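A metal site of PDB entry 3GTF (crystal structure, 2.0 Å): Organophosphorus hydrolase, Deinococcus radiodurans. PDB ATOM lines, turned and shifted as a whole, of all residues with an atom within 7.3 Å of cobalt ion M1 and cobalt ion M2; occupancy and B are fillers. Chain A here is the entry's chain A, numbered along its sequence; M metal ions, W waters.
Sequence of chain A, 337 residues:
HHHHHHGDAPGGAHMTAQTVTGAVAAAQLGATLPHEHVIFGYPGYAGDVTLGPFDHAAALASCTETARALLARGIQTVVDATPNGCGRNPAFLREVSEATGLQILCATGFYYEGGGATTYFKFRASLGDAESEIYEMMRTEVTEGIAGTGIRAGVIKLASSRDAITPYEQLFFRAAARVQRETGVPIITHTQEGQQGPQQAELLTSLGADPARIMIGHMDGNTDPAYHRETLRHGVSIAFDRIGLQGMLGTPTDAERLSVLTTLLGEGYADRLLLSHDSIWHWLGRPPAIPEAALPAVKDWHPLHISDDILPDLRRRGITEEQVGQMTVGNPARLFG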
ATOM      1  N   HIS A  35     -22.370 -10.772  -3.921  1.00  0.00           N
ATOM      2  CA  HIS A  35     -22.704  -9.963  -5.089  1.00  0.00           C
ATOM      3  C   HIS A  35     -24.162  -9.481  -5.047  1.00  0.00           C
ATOM      4  O   HIS A  35     -25.065 -10.186  -5.461  1.00  0.00           O
ATOM      5  CB  HIS A  35     -22.483 -10.744  -6.368  1.00  0.00           C
ATOM      6  CG  HIS A  35     -22.662  -9.929  -7.620  1.00  0.00           C
ATOM      7  ND1 HIS A  35     -21.766  -9.990  -8.675  1.00  0.00           N
ATOM      8  CD2 HIS A  35     -23.644  -9.091  -8.008  1.00  0.00           C
ATOM      9  CE1 HIS A  35     -22.202  -9.208  -9.653  1.00  0.00           C
ATOM     10  NE2 HIS A  35     -23.340  -8.654  -9.268  1.00  0.00           N
ATOM     11  N   GLU A  36     -24.339  -8.261  -4.528  1.00  0.00           N
ATOM     12  CA  GLU A  36     -25.642  -7.602  -4.410  1.00  0.00           C
ATOM     13  C   GLU A  36     -25.467  -6.110  -4.770  1.00  0.00           C
ATOM     14  O   GLU A  36     -24.341  -5.582  -4.874  1.00  0.00           O
ATOM     15  CB  GLU A  36     -26.150  -7.696  -2.959  1.00  0.00           C
ATOM     16  CG  GLU A  36     -26.197  -9.128  -2.398  1.00  0.00           C
ATOM     17  CD  GLU A  36     -27.235  -9.994  -3.063  1.00  0.00           C
ATOM     18  OE1 GLU A  36     -27.081 -11.225  -3.020  1.00  0.00           O
ATOM     19  OE2 GLU A  36     -28.206  -9.455  -3.613  1.00  0.00           O
ATOM     20  N   HIS A  37     -26.582  -5.416  -4.943  1.00  0.00           N
ATOM     21  CA  HIS A  37     -26.522  -3.994  -5.219  1.00  0.00           C
ATOM     22  C   HIS A  37     -27.552  -3.271  -4.325  1.00  0.00           C
ATOM     23  O   HIS A  37     -28.771  -3.454  -4.516  1.00  0.00           O
ATOM     24  CB  HIS A  37     -26.887  -3.762  -6.668  1.00  0.00           C
ATOM     25  CG  HIS A  37     -25.964  -4.420  -7.631  1.00  0.00           C
ATOM     26  ND1 HIS A  37     -24.698  -3.946  -7.898  1.00  0.00           N
ATOM     27  CD2 HIS A  37     -26.123  -5.533  -8.391  1.00  0.00           C
ATOM     28  CE1 HIS A  37     -24.119  -4.725  -8.791  1.00  0.00           C
ATOM     29  NE2 HIS A  37     -24.957  -5.701  -9.094  1.00  0.00           N
ATOM     30  N   PHE A  40     -28.811   0.829  -7.514  1.00  0.00           N
ATOM     31  CA  PHE A  40     -28.241   0.569  -8.816  1.00  0.00           C
ATOM     32  C   PHE A  40     -29.091   1.215  -9.880  1.00  0.00           C
ATOM     33  O   PHE A  40     -30.311   1.282  -9.758  1.00  0.00           O
ATOM     34  CB  PHE A  40     -28.179  -0.941  -9.045  1.00  0.00           C
ATOM     35  CG  PHE A  40     -27.625  -1.331 -10.387  1.00  0.00           C
ATOM     36  CD1 PHE A  40     -28.438  -1.360 -11.525  1.00  0.00           C
ATOM     37  CD2 PHE A  40     -26.294  -1.733 -10.511  1.00  0.00           C
ATOM     38  CE1 PHE A  40     -27.941  -1.766 -12.758  1.00  0.00           C
ATOM     39  CE2 PHE A  40     -25.774  -2.141 -11.779  1.00  0.00           C
ATOM     40  CZ  PHE A  40     -26.609  -2.159 -12.889  1.00  0.00           C
ATOM     41  N   ALA A  81     -21.420  -5.008  -5.680  1.00  0.00           N
ATOM     42  CA  ALA A  81     -20.683  -5.073  -6.931  1.00  0.00           C
ATOM     43  C   ALA A  81     -21.036  -3.995  -7.979  1.00  0.00           C
ATOM     44  O   ALA A  81     -20.672  -4.129  -9.176  1.00  0.00           O
ATOM     45  CB  ALA A  81     -20.861  -6.429  -7.533  1.00  0.00           C
ATOM     46  N   THR A  82     -21.699  -2.942  -7.541  1.00  0.00           N
ATOM     47  CA  THR A  82     -22.090  -1.847  -8.453  1.00  0.00           C
ATOM     48  C   THR A  82     -20.902  -1.111  -9.090  1.00  0.00           C
ATOM     49  O   THR A  82     -20.056  -0.610  -8.386  1.00  0.00           O
ATOM     50  CB  THR A  82     -22.953  -0.801  -7.670  1.00  0.00           C
ATOM     51  OG1 THR A  82     -24.022  -1.504  -6.999  1.00  0.00           O
ATOM     52  CG2 THR A  82     -23.572   0.261  -8.621  1.00  0.00           C
ATOM     53  N   PRO A  83     -20.822  -1.080 -10.432  1.00  0.00           N
ATOM     54  CA  PRO A  83     -19.758  -0.388 -11.183  1.00  0.00           C
ATOM     55  C   PRO A  83     -19.831   1.102 -10.914  1.00  0.00           C
ATOM     56  O   PRO A  83     -20.911   1.618 -10.659  1.00  0.00           O
ATOM     57  CB  PRO A  83     -20.090  -0.683 -12.629  1.00  0.00           C
ATOM     58  CG  PRO A  83     -20.749  -2.051 -12.546  1.00  0.00           C
ATOM     59  CD  PRO A  83     -21.556  -2.028 -11.304  1.00  0.00           C
ATOM     60  N   TYR A 111     -18.668  -1.442 -16.192  1.00  0.00           N
ATOM     61  CA  TYR A 111     -19.424  -2.561 -16.695  1.00  0.00           C
ATOM     62  C   TYR A 111     -18.959  -3.116 -18.043  1.00  0.00           C
ATOM     63  O   TYR A 111     -18.033  -2.565 -18.657  1.00  0.00           O
ATOM     64  CB  TYR A 111     -20.905  -2.194 -16.756  1.00  0.00           C
ATOM     65  CG  TYR A 111     -21.777  -3.341 -16.327  1.00  0.00           C
ATOM     66  CD1 TYR A 111     -21.216  -4.376 -15.575  1.00  0.00           C
ATOM     67  CD2 TYR A 111     -23.143  -3.373 -16.591  1.00  0.00           C
ATOM     68  CE1 TYR A 111     -21.992  -5.415 -15.083  1.00  0.00           C
ATOM     69  CE2 TYR A 111     -23.930  -4.414 -16.086  1.00  0.00           C
ATOM     70  CZ  TYR A 111     -23.339  -5.427 -15.337  1.00  0.00           C
ATOM     71  OH  TYR A 111     -24.088  -6.458 -14.799  1.00  0.00           O
ATOM     72  N   TYR A 112     -19.587  -4.197 -18.506  1.00  0.00           N
ATOM     73  CA  TYR A 112     -19.207  -4.806 -19.780  1.00  0.00           C
ATOM     74  C   TYR A 112     -19.553  -3.865 -20.925  1.00  0.00           C
ATOM     75  O   TYR A 112     -20.436  -3.021 -20.806  1.00  0.00           O
ATOM     76  CB  TYR A 112     -19.841  -6.198 -19.942  1.00  0.00           C
ATOM     77  CG  TYR A 112     -21.324  -6.259 -20.267  1.00  0.00           C
ATOM     78  CD1 TYR A 112     -21.755  -6.584 -21.559  1.00  0.00           C
ATOM     79  CD2 TYR A 112     -22.286  -6.011 -19.284  1.00  0.00           C
ATOM     80  CE1 TYR A 112     -23.109  -6.682 -21.861  1.00  0.00           C
ATOM     81  CE2 TYR A 112     -23.641  -6.089 -19.575  1.00  0.00           C
ATOM     82  CZ  TYR A 112     -24.043  -6.430 -20.853  1.00  0.00           C
ATOM     83  OH  TYR A 112     -25.388  -6.574 -21.132  1.00  0.00           O
ATOM     84  N   KCX A 157     -14.321  -4.917  -9.604  1.00  0.00           N
ATOM     85  CA  KCX A 157     -15.363  -5.554 -10.381  1.00  0.00           C
ATOM     86  CB  KCX A 157     -16.736  -4.854 -10.097  1.00  0.00           C
ATOM     87  CG  KCX A 157     -17.928  -5.153 -11.066  1.00  0.00           C
ATOM     88  CD  KCX A 157     -18.386  -6.624 -10.992  1.00  0.00           C
ATOM     89  CE  KCX A 157     -19.624  -6.913 -11.884  1.00  0.00           C
ATOM     90  NZ  KCX A 157     -20.811  -6.236 -11.356  1.00  0.00           N
ATOM     91  C   KCX A 157     -14.954  -5.472 -11.854  1.00  0.00           C
ATOM     92  O   KCX A 157     -14.617  -4.393 -12.367  1.00  0.00           O
ATOM     93  CX  KCX A 157     -22.057  -6.505 -11.760  1.00  0.00           C
ATOM     94  OQ1 KCX A 157     -22.306  -7.458 -12.547  1.00  0.00           O
ATOM     95  OQ2 KCX A 157     -23.043  -5.893 -11.257  1.00  0.00           O
ATOM     96  N   LEU A 158     -14.998  -6.610 -12.524  1.00  0.00           N
ATOM     97  CA  LEU A 158     -14.641  -6.744 -13.936  1.00  0.00           C
ATOM     98  C   LEU A 158     -15.858  -7.327 -14.653  1.00  0.00           C
ATOM     99  O   LEU A 158     -16.644  -8.016 -14.013  1.00  0.00           O
ATOM    100  CB  LEU A 158     -13.466  -7.694 -14.080  1.00  0.00           C
ATOM    101  CG  LEU A 158     -12.108  -7.198 -13.553  1.00  0.00           C
ATOM    102  CD1 LEU A 158     -10.979  -8.228 -13.904  1.00  0.00           C
ATOM    103  CD2 LEU A 158     -11.803  -5.834 -14.223  1.00  0.00           C
ATOM    104  N   ALA A 159     -16.052  -7.043 -15.941  1.00  0.00           N
ATOM    105  CA  ALA A 159     -17.217  -7.588 -16.670  1.00  0.00           C
ATOM    106  C   ALA A 159     -16.876  -7.820 -18.147  1.00  0.00           C
ATOM    107  O   ALA A 159     -16.173  -7.040 -18.736  1.00  0.00           O
ATOM    108  CB  ALA A 159     -18.390  -6.604 -16.565  1.00  0.00           C
ATOM    109  N   THR A 189     -16.300 -10.968 -10.853  1.00  0.00           N
ATOM    110  CA  THR A 189     -16.652 -10.637 -12.188  1.00  0.00           C
ATOM    111  C   THR A 189     -18.111 -10.906 -12.554  1.00  0.00           C
ATOM    112  O   THR A 189     -18.864 -11.551 -11.807  1.00  0.00           O
ATOM    113  CB  THR A 189     -15.737 -11.377 -13.177  1.00  0.00           C
ATOM    114  OG1 THR A 189     -16.161 -12.738 -13.336  1.00  0.00           O
ATOM    115  CG2 THR A 189     -14.356 -11.395 -12.646  1.00  0.00           C
ATOM    116  N   HIS A 190     -18.474 -10.369 -13.719  1.00  0.00           N
ATOM    117  CA  HIS A 190     -19.770 -10.542 -14.313  1.00  0.00           C
ATOM    118  C   HIS A 190     -19.428 -11.263 -15.605  1.00  0.00           C
ATOM    119  O   HIS A 190     -18.428 -10.920 -16.256  1.00  0.00           O
ATOM    120  CB  HIS A 190     -20.379  -9.145 -14.625  1.00  0.00           C
ATOM    121  CG  HIS A 190     -21.362  -9.119 -15.767  1.00  0.00           C
ATOM    122  ND1 HIS A 190     -22.696  -8.809 -15.597  1.00  0.00           N
ATOM    123  CD2 HIS A 190     -21.179  -9.227 -17.121  1.00  0.00           C
ATOM    124  CE1 HIS A 190     -23.297  -8.723 -16.773  1.00  0.00           C
ATOM    125  NE2 HIS A 190     -22.397  -8.977 -17.718  1.00  0.00           N
ATOM    126  N   THR A 191     -20.204 -12.291 -15.940  1.00  0.00           N
ATOM    127  CA  THR A 191     -20.053 -12.951 -17.228  1.00  0.00           C
ATOM    128  C   THR A 191     -21.429 -12.700 -17.848  1.00  0.00           C
ATOM    129  O   THR A 191     -22.444 -12.659 -17.139  1.00  0.00           O
ATOM    130  CB  THR A 191     -19.801 -14.473 -17.133  1.00  0.00           C
ATOM    131  OG1 THR A 191     -20.809 -15.081 -16.317  1.00  0.00           O
ATOM    132  CG2 THR A 191     -18.410 -14.737 -16.578  1.00  0.00           C
ATOM    133  N   GLN A 192     -21.451 -12.503 -19.160  1.00  0.00           N
ATOM    134  CA  GLN A 192     -22.692 -12.232 -19.862  1.00  0.00           C
ATOM    135  C   GLN A 192     -23.262 -13.509 -20.447  1.00  0.00           C
ATOM    136  O   GLN A 192     -22.531 -14.305 -21.040  1.00  0.00           O
ATOM    137  CB  GLN A 192     -22.409 -11.250 -20.985  1.00  0.00           C
ATOM    138  CG  GLN A 192     -23.602 -10.890 -21.815  1.00  0.00           C
ATOM    139  CD  GLN A 192     -24.615 -10.058 -21.041  1.00  0.00           C
ATOM    140  OE1 GLN A 192     -24.342  -9.500 -19.963  1.00  0.00           O
ATOM    141  NE2 GLN A 192     -25.803  -9.954 -21.613  1.00  0.00           N
ATOM    142  N   GLY A 217     -18.142 -14.488 -11.760  1.00  0.00           N
ATOM    143  CA  GLY A 217     -19.572 -14.380 -11.481  1.00  0.00           C
ATOM    144  C   GLY A 217     -20.557 -14.777 -12.551  1.00  0.00           C
ATOM    145  O   GLY A 217     -20.185 -15.059 -13.711  1.00  0.00           O
ATOM    146  N   HIS A 218     -21.823 -14.753 -12.159  1.00  0.00           N
ATOM    147  CA  HIS A 218     -22.941 -15.129 -13.027  1.00  0.00           C
ATOM    148  C   HIS A 218     -22.726 -16.491 -13.649  1.00  0.00           C
ATOM    149  O   HIS A 218     -23.200 -16.750 -14.741  1.00  0.00           O
ATOM    150  CB  HIS A 218     -23.160 -14.113 -14.133  1.00  0.00           C
ATOM    151  CG  HIS A 218     -23.267 -12.719 -13.629  1.00  0.00           C
ATOM    152  ND1 HIS A 218     -23.548 -12.428 -12.320  1.00  0.00           N
ATOM    153  CD2 HIS A 218     -23.183 -11.532 -14.279  1.00  0.00           C
ATOM    154  CE1 HIS A 218     -23.633 -11.115 -12.169  1.00  0.00           C
ATOM    155  NE2 HIS A 218     -23.415 -10.556 -13.339  1.00  0.00           N
ATOM    156  N   ASP A 241     -24.553 -16.360  -8.801  1.00  0.00           N
ATOM    157  CA  ASP A 241     -24.951 -15.152  -8.111  1.00  0.00           C
ATOM    158  C   ASP A 241     -26.164 -14.374  -8.494  1.00  0.00           C
ATOM    159  O   ASP A 241     -26.304 -13.223  -8.096  1.00  0.00           O
ATOM    160  CB  ASP A 241     -23.761 -14.203  -7.991  1.00  0.00           C
ATOM    161  CG  ASP A 241     -23.161 -13.846  -9.322  1.00  0.00           C
ATOM    162  OD1 ASP A 241     -22.041 -13.281  -9.329  1.00  0.00           O
ATOM    163  OD2 ASP A 241     -23.808 -14.143 -10.359  1.00  0.00           O
ATOM    164  N   ARG A 242     -27.046 -14.974  -9.263  1.00  0.00           N
ATOM    165  CA  ARG A 242     -28.243 -14.240  -9.586  1.00  0.00           C
ATOM    166  C   ARG A 242     -29.392 -15.188  -9.225  1.00  0.00           C
ATOM    167  O   ARG A 242     -30.368 -15.306  -9.979  1.00  0.00           O
ATOM    168  CB  ARG A 242     -28.244 -13.912 -11.072  1.00  0.00           C
ATOM    169  CG  ARG A 242     -26.968 -13.236 -11.519  1.00  0.00           C
ATOM    170  CD  ARG A 242     -27.062 -12.855 -12.988  1.00  0.00           C
ATOM    171  NE  ARG A 242     -27.710 -11.559 -13.138  1.00  0.00           N
ATOM    172  CZ  ARG A 242     -28.163 -11.080 -14.301  1.00  0.00           C
ATOM    173  NH1 ARG A 242     -28.033 -11.795 -15.398  1.00  0.00           N
ATOM    174  NH2 ARG A 242     -28.747  -9.889 -14.354  1.00  0.00           N
ATOM    175  N   HIS A 277     -27.582 -13.196  -5.024  1.00  0.00           N
ATOM    176  CA  HIS A 277     -28.789 -12.915  -5.795  1.00  0.00           C
ATOM    177  C   HIS A 277     -28.599 -11.819  -6.872  1.00  0.00           C
ATOM    178  O   HIS A 277     -29.374 -11.740  -7.801  1.00  0.00           O
ATOM    179  CB  HIS A 277     -29.978 -12.453  -4.888  1.00  0.00           C
ATOM    180  CG  HIS A 277     -30.065 -13.140  -3.550  1.00  0.00           C
ATOM    181  ND1 HIS A 277     -30.968 -14.144  -3.282  1.00  0.00           N
ATOM    182  CD2 HIS A 277     -29.415 -12.902  -2.392  1.00  0.00           C
ATOM    183  CE1 HIS A 277     -30.863 -14.519  -2.018  1.00  0.00           C
ATOM    184  NE2 HIS A 277     -29.928 -13.777  -1.454  1.00  0.00           N
ATOM    185  N   ASP A 278     -27.600 -10.956  -6.724  1.00  0.00           N
ATOM    186  CA  ASP A 278     -27.418  -9.842  -7.664  1.00  0.00           C
ATOM    187  C   ASP A 278     -28.700  -8.985  -7.582  1.00  0.00           C
ATOM    188  O   ASP A 278     -29.173  -8.444  -8.580  1.00  0.00           O
ATOM    189  CB  ASP A 278     -27.240 -10.391  -9.085  1.00  0.00           C
ATOM    190  CG  ASP A 278     -26.814  -9.326 -10.074  1.00  0.00           C
ATOM    191  OD1 ASP A 278     -26.929  -9.562 -11.299  1.00  0.00           O
ATOM    192  OD2 ASP A 278     -26.366  -8.268  -9.618  1.00  0.00           O
ATOM    193  N   SER A 279     -29.274  -8.854  -6.383  1.00  0.00           N
ATOM    194  CA  SER A 279     -30.519  -8.092  -6.226  1.00  0.00           C
ATOM    195  C   SER A 279     -30.281  -6.602  -6.139  1.00  0.00           C
ATOM    196  O   SER A 279     -29.202  -6.163  -5.801  1.00  0.00           O
ATOM    197  CB  SER A 279     -31.265  -8.543  -4.959  1.00  0.00           C
ATOM    198  OG  SER A 279     -30.626  -8.049  -3.796  1.00  0.00           O
ATOM    199  N   ILE A 280     -31.307  -5.807  -6.472  1.00  0.00           N
ATOM    200  CA  ILE A 280     -31.200  -4.358  -6.363  1.00  0.00           C
ATOM    201  C   ILE A 280     -32.180  -3.983  -5.263  1.00  0.00           C
ATOM    202  O   ILE A 280     -33.403  -4.188  -5.399  1.00  0.00           O
ATOM    203  CB  ILE A 280     -31.605  -3.631  -7.676  1.00  0.00           C
ATOM    204  CG1 ILE A 280     -30.577  -3.907  -8.759  1.00  0.00           C
ATOM    205  CG2 ILE A 280     -31.666  -2.121  -7.447  1.00  0.00           C
ATOM    206  CD1 ILE A 280     -30.996  -4.971  -9.700  1.00  0.00           C
HETATM  207 CO    CO M   1     -24.608  -7.135 -10.447  1.00  0.00          CO
HETATM  208 CO    CO M   2     -23.634  -8.391 -13.696  1.00  0.00          CO
HETATM  209  O   HOH W   1     -25.706  -8.877 -14.693  1.00  0.00           O
HETATM  210  O   HOH W   2     -25.135  -8.026 -11.942  1.00  0.00           O
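Cobalt ion M1 is bound by water W2 (1.8 Å).
NE2 of His 37 binds cobalt ion M1 (2.0 Å).
OQ2 of KCX 157 binds cobalt ion M1 (2.2 Å).
OD2 of Asp 278 binds cobalt ion M1 (2.2 Å).
Cobalt ion M1 is bound by NE2 of His 35, 2.3 Å away.
The nearest printed residue that does not touch cobalt ion M2 is Asp 278 (4.2 Å).
NZ of KCX 157 sits close to O of Ala 81.
OD1 of Asp 278 is in salt-bridge range of NE of Arg 242, 2.8 Å away.
The backbone NH (N) of His 37 sits at hydrogen-bond distance from the backbone carbonyl oxygen (O) of Ser 279, at 2.9 Å.
A ring nitrogen (ND1) of His 218 lies within hydrogen-bond range of the side-chain carboxylate (OD2) of Asp 241 (2.6 Å).
The backbone NH (N) of His 190 is in hydrogen-bond range of the backbone carbonyl oxygen (O) of Leu 158 (3.0 Å).
A ring nitrogen (ND1) of His 35 sits at hydrogen-bond distance from the side-chain carboxylate (OD1) of Asp 241 (3.4 Å).
The backbone NH (N) of Asp 278 sits at hydrogen-bond distance from the backbone carbonyl oxygen (O) of Asp 241 (2.9 Å).
OE1 of Gln 192 sits at hydrogen-bond distance from NE2 of His 190.
Cobalt ion M2 is bound by OQ1 of KCX 157 (2.0 Å), a ring nitrogen (ND1) of His 190 (2.2 Å), a ring nitrogen (NE2) of His 218 (2.2 Å), the side-chain hydroxyl (OH) of Tyr 111 (2.3 Å), water W2 (2.3 Å) and water W1 (2.4 Å).
Of the 24 residues printed, 4 come within 4 Å of cobalt ion M1.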
